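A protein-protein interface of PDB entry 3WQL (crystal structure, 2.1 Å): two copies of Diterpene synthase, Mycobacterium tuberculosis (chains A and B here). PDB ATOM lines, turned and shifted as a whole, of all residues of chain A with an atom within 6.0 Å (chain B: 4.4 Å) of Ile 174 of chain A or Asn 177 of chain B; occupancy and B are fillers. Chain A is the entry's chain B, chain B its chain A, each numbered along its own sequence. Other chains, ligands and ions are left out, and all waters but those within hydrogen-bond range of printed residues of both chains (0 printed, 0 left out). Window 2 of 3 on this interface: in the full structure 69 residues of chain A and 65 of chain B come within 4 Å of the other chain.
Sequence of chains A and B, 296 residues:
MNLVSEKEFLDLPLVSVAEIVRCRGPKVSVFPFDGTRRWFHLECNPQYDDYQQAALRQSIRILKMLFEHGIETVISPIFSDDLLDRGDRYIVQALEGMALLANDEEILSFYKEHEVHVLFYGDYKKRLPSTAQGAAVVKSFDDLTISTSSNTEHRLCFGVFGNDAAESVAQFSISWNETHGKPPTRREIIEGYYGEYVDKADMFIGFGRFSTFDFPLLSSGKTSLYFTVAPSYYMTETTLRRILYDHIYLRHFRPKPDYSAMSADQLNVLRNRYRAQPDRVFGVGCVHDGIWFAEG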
ATOM      1  N   VAL A 169      12.802 -22.150  27.825  1.00  0.00           N
ATOM      2  CA  VAL A 169      12.215 -23.485  27.709  1.00  0.00           C
ATOM      3  C   VAL A 169      11.123 -23.502  26.635  1.00  0.00           C
ATOM      4  O   VAL A 169      10.940 -24.495  25.938  1.00  0.00           O
ATOM      5  CB  VAL A 169      11.578 -23.959  29.041  1.00  0.00           C
ATOM      6  CG1 VAL A 169      10.834 -25.260  28.811  1.00  0.00           C
ATOM      7  CG2 VAL A 169      12.652 -24.157  30.111  1.00  0.00           C
ATOM      8  N   ALA A 170      10.386 -22.407  26.511  1.00  0.00           N
ATOM      9  CA  ALA A 170       9.324 -22.340  25.504  1.00  0.00           C
ATOM     10  C   ALA A 170       9.928 -22.464  24.092  1.00  0.00           C
ATOM     11  O   ALA A 170       9.514 -23.301  23.286  1.00  0.00           O
ATOM     12  CB  ALA A 170       8.577 -21.035  25.637  1.00  0.00           C
ATOM     13  N   GLN A 171      10.924 -21.638  23.808  1.00  0.00           N
ATOM     14  CA  GLN A 171      11.575 -21.647  22.511  1.00  0.00           C
ATOM     15  C   GLN A 171      12.300 -22.961  22.229  1.00  0.00           C
ATOM     16  O   GLN A 171      12.169 -23.524  21.142  1.00  0.00           O
ATOM     17  CB  GLN A 171      12.521 -20.452  22.431  1.00  0.00           C
ATOM     18  CG  GLN A 171      11.764 -19.170  22.752  1.00  0.00           C
ATOM     19  CD  GLN A 171      12.594 -17.924  22.601  1.00  0.00           C
ATOM     20  OE1 GLN A 171      12.148 -16.827  22.951  1.00  0.00           O
ATOM     21  NE2 GLN A 171      13.805 -18.076  22.071  1.00  0.00           N
ATOM     22  N   PHE A 172      13.059 -23.451  23.204  1.00  0.00           N
ATOM     23  CA  PHE A 172      13.755 -24.719  23.045  1.00  0.00           C
ATOM     24  C   PHE A 172      12.738 -25.792  22.646  1.00  0.00           C
ATOM     25  O   PHE A 172      12.961 -26.558  21.713  1.00  0.00           O
ATOM     26  CB  PHE A 172      14.420 -25.136  24.362  1.00  0.00           C
ATOM     27  CG  PHE A 172      14.880 -26.572  24.378  1.00  0.00           C
ATOM     28  CD1 PHE A 172      16.106 -26.935  23.827  1.00  0.00           C
ATOM     29  CD2 PHE A 172      14.063 -27.571  24.905  1.00  0.00           C
ATOM     30  CE1 PHE A 172      16.510 -28.264  23.800  1.00  0.00           C
ATOM     31  CE2 PHE A 172      14.452 -28.892  24.884  1.00  0.00           C
ATOM     32  CZ  PHE A 172      15.680 -29.246  24.330  1.00  0.00           C
ATOM     33  N   SER A 173      11.623 -25.833  23.369  1.00  0.00           N
ATOM     34  CA  SER A 173      10.570 -26.816  23.139  1.00  0.00           C
ATOM     35  C   SER A 173       9.943 -26.750  21.752  1.00  0.00           C
ATOM     36  O   SER A 173       9.687 -27.776  21.126  1.00  0.00           O
ATOM     37  CB  SER A 173       9.483 -26.666  24.206  1.00  0.00           C
ATOM     38  OG  SER A 173      10.005 -26.951  25.494  1.00  0.00           O
ATOM     39  N   ILE A 174       9.677 -25.543  21.278  1.00  0.00           N
ATOM     40  CA  ILE A 174       9.094 -25.377  19.962  1.00  0.00           C
ATOM     41  C   ILE A 174      10.044 -25.946  18.898  1.00  0.00           C
ATOM     42  O   ILE A 174       9.631 -26.746  18.058  1.00  0.00           O
ATOM     43  CB  ILE A 174       8.791 -23.891  19.692  1.00  0.00           C
ATOM     44  CG1 ILE A 174       7.773 -23.391  20.724  1.00  0.00           C
ATOM     45  CG2 ILE A 174       8.223 -23.715  18.289  1.00  0.00           C
ATOM     46  CD1 ILE A 174       7.576 -21.892  20.736  1.00  0.00           C
ATOM     47  N   SER A 175      11.317 -25.562  18.946  1.00  0.00           N
ATOM     48  CA  SER A 175      12.282 -26.075  17.975  1.00  0.00           C
ATOM     49  C   SER A 175      12.377 -27.592  18.085  1.00  0.00           C
ATOM     50  O   SER A 175      12.314 -28.307  17.085  1.00  0.00           O
ATOM     51  CB  SER A 175      13.665 -25.470  18.211  1.00  0.00           C
ATOM     52  OG  SER A 175      13.642 -24.065  18.035  1.00  0.00           O
ATOM     53  N   TRP A 176      12.526 -28.082  19.309  1.00  0.00           N
ATOM     54  CA  TRP A 176      12.637 -29.514  19.530  1.00  0.00           C
ATOM     55  C   TRP A 176      11.516 -30.296  18.858  1.00  0.00           C
ATOM     56  O   TRP A 176      11.773 -31.235  18.110  1.00  0.00           O
ATOM     57  CB  TRP A 176      12.652 -29.821  21.023  1.00  0.00           C
ATOM     58  CG  TRP A 176      12.818 -31.274  21.311  1.00  0.00           C
ATOM     59  CD1 TRP A 176      11.832 -32.217  21.390  1.00  0.00           C
ATOM     60  CD2 TRP A 176      14.051 -31.962  21.525  1.00  0.00           C
ATOM     61  NE1 TRP A 176      12.378 -33.453  21.642  1.00  0.00           N
ATOM     62  CE2 TRP A 176      13.740 -33.326  21.728  1.00  0.00           C
ATOM     63  CE3 TRP A 176      15.395 -31.558  21.567  1.00  0.00           C
ATOM     64  CZ2 TRP A 176      14.723 -34.290  21.969  1.00  0.00           C
ATOM     65  CZ3 TRP A 176      16.374 -32.516  21.810  1.00  0.00           C
ATOM     66  CH2 TRP A 176      16.031 -33.867  22.006  1.00  0.00           C
ATOM     67  N   ASN A 177      10.277 -29.911  19.136  1.00  0.00           N
ATOM     68  CA  ASN A 177       9.112 -30.575  18.561  1.00  0.00           C
ATOM     69  C   ASN A 177       9.131 -30.532  17.032  1.00  0.00           C
ATOM     70  O   ASN A 177       8.722 -31.482  16.362  1.00  0.00           O
ATOM     71  CB  ASN A 177       7.835 -29.914  19.075  1.00  0.00           C
ATOM     72  CG  ASN A 177       6.592 -30.480  18.435  1.00  0.00           C
ATOM     73  OD1 ASN A 177       5.930 -29.814  17.633  1.00  0.00           O
ATOM     74  ND2 ASN A 177       6.269 -31.721  18.775  1.00  0.00           N
ATOM     75  N   GLU A 178       9.617 -29.420  16.491  1.00  0.00           N
ATOM     76  CA  GLU A 178       9.700 -29.228  15.053  1.00  0.00           C
ATOM     77  C   GLU A 178      10.650 -30.243  14.410  1.00  0.00           C
ATOM     78  O   GLU A 178      10.333 -30.836  13.376  1.00  0.00           O
ATOM     79  CB  GLU A 178      10.179 -27.801  14.766  1.00  0.00           C
ATOM     80  CG  GLU A 178       9.740 -27.236  13.426  1.00  0.00           C
ATOM     81  CD  GLU A 178      10.506 -27.812  12.257  1.00  0.00           C
ATOM     82  OE1 GLU A 178      10.163 -27.470  11.105  1.00  0.00           O
ATOM     83  OE2 GLU A 178      11.452 -28.597  12.482  1.00  0.00           O
ATOM     84  N   THR A 179      11.809 -30.450  15.031  1.00  0.00           N
ATOM     85  CA  THR A 179      12.801 -31.372  14.493  1.00  0.00           C
ATOM     86  C   THR A 179      12.648 -32.814  14.975  1.00  0.00           C
ATOM     87  O   THR A 179      13.339 -33.704  14.479  1.00  0.00           O
ATOM     88  CB  THR A 179      14.240 -30.917  14.831  1.00  0.00           C
ATOM     89  OG1 THR A 179      14.530 -31.233  16.195  1.00  0.00           O
ATOM     90  CG2 THR A 179      14.393 -29.422  14.632  1.00  0.00           C
ATOM     91  N   SER B 173       3.855 -24.318  25.332  1.00  0.00           N
ATOM     92  CA  SER B 173       4.567 -23.472  24.388  1.00  0.00           C
ATOM     93  C   SER B 173       4.444 -23.976  22.954  1.00  0.00           C
ATOM     94  O   SER B 173       4.287 -23.188  22.024  1.00  0.00           O
ATOM     95  CB  SER B 173       6.037 -23.375  24.798  1.00  0.00           C
ATOM     96  OG  SER B 173       6.137 -22.777  26.080  1.00  0.00           O
ATOM     97  N   ILE B 174       4.510 -25.290  22.788  1.00  0.00           N
ATOM     98  CA  ILE B 174       4.398 -25.903  21.474  1.00  0.00           C
ATOM     99  C   ILE B 174       2.993 -25.679  20.911  1.00  0.00           C
ATOM    100  O   ILE B 174       2.832 -25.390  19.723  1.00  0.00           O
ATOM    101  CB  ILE B 174       4.709 -27.415  21.562  1.00  0.00           C
ATOM    102  CG1 ILE B 174       6.201 -27.600  21.860  1.00  0.00           C
ATOM    103  CG2 ILE B 174       4.300 -28.129  20.265  1.00  0.00           C
ATOM    104  CD1 ILE B 174       6.587 -29.012  22.259  1.00  0.00           C
ATOM    105  N   SER B 175       1.978 -25.807  21.765  1.00  0.00           N
ATOM    106  CA  SER B 175       0.606 -25.601  21.318  1.00  0.00           C
ATOM    107  C   SER B 175       0.432 -24.127  21.007  1.00  0.00           C
ATOM    108  O   SER B 175      -0.137 -23.756  19.980  1.00  0.00           O
ATOM    109  CB  SER B 175      -0.396 -26.016  22.399  1.00  0.00           C
ATOM    110  OG  SER B 175      -0.269 -27.389  22.724  1.00  0.00           O
ATOM    111  N   TRP B 176       0.941 -23.282  21.894  1.00  0.00           N
ATOM    112  CA  TRP B 176       0.828 -21.845  21.705  1.00  0.00           C
ATOM    113  C   TRP B 176       1.442 -21.380  20.389  1.00  0.00           C
ATOM    114  O   TRP B 176       0.883 -20.514  19.713  1.00  0.00           O
ATOM    115  CB  TRP B 176       1.489 -21.099  22.863  1.00  0.00           C
ATOM    116  CG  TRP B 176       1.317 -19.616  22.768  1.00  0.00           C
ATOM    117  CD1 TRP B 176       2.041 -18.748  21.998  1.00  0.00           C
ATOM    118  CD2 TRP B 176       0.345 -18.824  23.461  1.00  0.00           C
ATOM    119  NE1 TRP B 176       1.585 -17.459  22.177  1.00  0.00           N
ATOM    120  CE2 TRP B 176       0.543 -17.479  23.069  1.00  0.00           C
ATOM    121  CE3 TRP B 176      -0.676 -19.122  24.376  1.00  0.00           C
ATOM    122  CZ2 TRP B 176      -0.245 -16.426  23.567  1.00  0.00           C
ATOM    123  CZ3 TRP B 176      -1.458 -18.077  24.869  1.00  0.00           C
ATOM    124  CH2 TRP B 176      -1.236 -16.746  24.462  1.00  0.00           C
ATOM    125  N   ASN B 177       2.595 -21.937  20.029  1.00  0.00           N
ATOM    126  CA  ASN B 177       3.247 -21.541  18.790  1.00  0.00           C
ATOM    127  C   ASN B 177       2.387 -21.942  17.597  1.00  0.00           C
ATOM    128  O   ASN B 177       2.391 -21.275  16.570  1.00  0.00           O
ATOM    129  CB  ASN B 177       4.628 -22.188  18.669  1.00  0.00           C
ATOM    130  CG  ASN B 177       5.353 -21.766  17.399  1.00  0.00           C
ATOM    131  OD1 ASN B 177       5.515 -22.554  16.466  1.00  0.00           O
ATOM    132  ND2 ASN B 177       5.777 -20.510  17.355  1.00  0.00           N
ATOM    133  N   GLU B 178       1.641 -23.031  17.745  1.00  0.00           N
ATOM    134  CA  GLU B 178       0.775 -23.504  16.679  1.00  0.00           C
ATOM    135  C   GLU B 178      -0.451 -22.603  16.529  1.00  0.00           C
ATOM    136  O   GLU B 178      -0.902 -22.341  15.423  1.00  0.00           O
ATOM    137  CB  GLU B 178       0.339 -24.942  16.967  1.00  0.00           C
ATOM    138  CG  GLU B 178       1.510 -25.902  17.129  1.00  0.00           C
ATOM    139  CD  GLU B 178       1.076 -27.318  17.460  1.00  0.00           C
ATOM    140  OE1 GLU B 178       0.242 -27.489  18.375  1.00  0.00           O
ATOM    141  OE2 GLU B 178       1.580 -28.261  16.811  1.00  0.00           O
ATOM    142  N   THR B 179      -0.976 -22.115  17.647  1.00  0.00           N
ATOM    143  CA  THR B 179      -2.156 -21.264  17.612  1.00  0.00           C
ATOM    144  C   THR B 179      -1.827 -19.788  17.432  1.00  0.00           C
ATOM    145  O   THR B 179      -2.735 -18.965  17.313  1.00  0.00           O
ATOM    146  CB  THR B 179      -2.992 -21.419  18.900  1.00  0.00           C
ATOM    147  OG1 THR B 179      -2.199 -21.043  20.036  1.00  0.00           O
ATOM    148  CG2 THR B 179      -3.462 -22.873  19.064  1.00  0.00           C
ATOM    149  N   HIS B 180      -0.541 -19.449  17.405  1.00  0.00           N
ATOM    150  CA  HIS B 180      -0.128 -18.050  17.247  1.00  0.00           C
ATOM    151  C   HIS B 180       0.971 -17.798  16.216  1.00  0.00           C
ATOM    152  O   HIS B 180       1.086 -16.691  15.695  1.00  0.00           O
ATOM    153  CB  HIS B 180       0.359 -17.478  18.583  1.00  0.00           C
ATOM    154  CG  HIS B 180      -0.721 -17.320  19.608  1.00  0.00           C
ATOM    155  ND1 HIS B 180      -1.249 -18.385  20.307  1.00  0.00           N
ATOM    156  CD2 HIS B 180      -1.384 -16.220  20.037  1.00  0.00           C
ATOM    157  CE1 HIS B 180      -2.191 -17.947  21.123  1.00  0.00           C
ATOM    158  NE2 HIS B 180      -2.293 -16.638  20.978  1.00  0.00           N
ATOM    159  N   GLY B 181       1.787 -18.808  15.938  1.00  0.00           N
ATOM    160  CA  GLY B 181       2.877 -18.626  14.996  1.00  0.00           C
ATOM    161  C   GLY B 181       4.060 -17.964  15.690  1.00  0.00           C
ATOM    162  O   GLY B 181       5.054 -17.598  15.054  1.00  0.00           O
ATOM    163  N   LYS B 182       3.951 -17.808  17.007  1.00  0.00           N
ATOM    164  CA  LYS B 182       5.008 -17.198  17.815  1.00  0.00           C
ATOM    165  C   LYS B 182       5.121 -17.928  19.144  1.00  0.00           C
ATOM    166  O   LYS B 182       4.180 -18.588  19.580  1.00  0.00           O
ATOM    167  CB  LYS B 182       4.684 -15.744  18.162  1.00  0.00           C
ATOM    168  CG  LYS B 182       4.482 -14.796  17.018  1.00  0.00           C
ATOM    169  CD  LYS B 182       4.239 -13.393  17.568  1.00  0.00           C
ATOM    170  CE  LYS B 182       3.124 -13.405  18.613  1.00  0.00           C
ATOM    171  NZ  LYS B 182       2.882 -12.074  19.238  1.00  0.00           N
ATOM    172  N   PRO B 183       6.286 -17.827  19.801  1.00  0.00           N
ATOM    173  CA  PRO B 183       6.424 -18.498  21.093  1.00  0.00           C
ATOM    174  C   PRO B 183       5.760 -17.566  22.107  1.00  0.00           C
ATOM    175  O   PRO B 183       5.698 -16.353  21.890  1.00  0.00           O
ATOM    176  CB  PRO B 183       7.935 -18.589  21.278  1.00  0.00           C
ATOM    177  CG  PRO B 183       8.424 -17.337  20.603  1.00  0.00           C
ATOM    178  CD  PRO B 183       7.582 -17.291  19.337  1.00  0.00           C
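CB of Ala 170 of chain A touches OG of Ser 173 of chain B (3.0 Å). Ile 174 of chain B touches Ser 173 of chain A (CD1 to O, 3.5 Å). O of Ser 173 of chain B touches CG1 of Ile 174 of chain A, 3.7 Å away. Ile 174 of chain A touches Asn 177 of chain B (CG2 to OD1, 3.5 Å). Pro 183 of chain B touches Ile 174 of chain A (CB to CD1, 3.4 Å). OD1 of Asn 177 of chain A touches CG2 of Ile 174 of chain B, 3.5 Å away.
N of Lys 182 of chain B sits close to ND2 of Asn 177 of chain B, 3.3 Å away. The side-chain hydroxyl (OG) of Ser 173 of chain A sits at hydrogen-bond distance from the backbone carbonyl oxygen (O) of Val 169 of chain A (2.7 Å).
Ser 173 of chain A touches Ile 174 of chain B, and with the chains exchanged Ile 174 of chain A touches Ser 173 of chain B. Ile 174 of chain A touches Asn 177 of chain B, and with the chains exchanged Asn 177 of chain A touches Ile 174 of chain B. Positions printed for both chains: 173, 174, 175, 176, 177, 178 and 179.
Printed residues of chain B that touch a printed residue of chain A: Ser 173, Ile 174, Asn 177 and Pro 183. Along chain A the printed residues that touch a printed residue of chain B span positions 170 to 177. Among the printed residues, 6 pairs touch across the chains.
Printed residues of chain B within 4 Å of Ala 170 of chain A: Ser 173. Printed residues of chain A within 4 Å of Ser 173 of chain B: Ala 170 (3.0 Å) and Ile 174 (3.7 Å). Of the printed residues of chain A, Ile 174 of chain B touches Ser 173 (3.5 Å) and Asn 177 (3.5 Å). Asn 177 of chain B touches just one residue of chain A: Ile 174 (3.5 Å). Lys 182 of chain B touches none of the printed residues of chain A. Of the printed residues of chain A, Pro 183 of chain B touches Ile 174 (3.4 Å). The nearest printed residue of chain B that does not touch Asn 177 of chain A is Glu 178 of chain B (4.7 Å).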
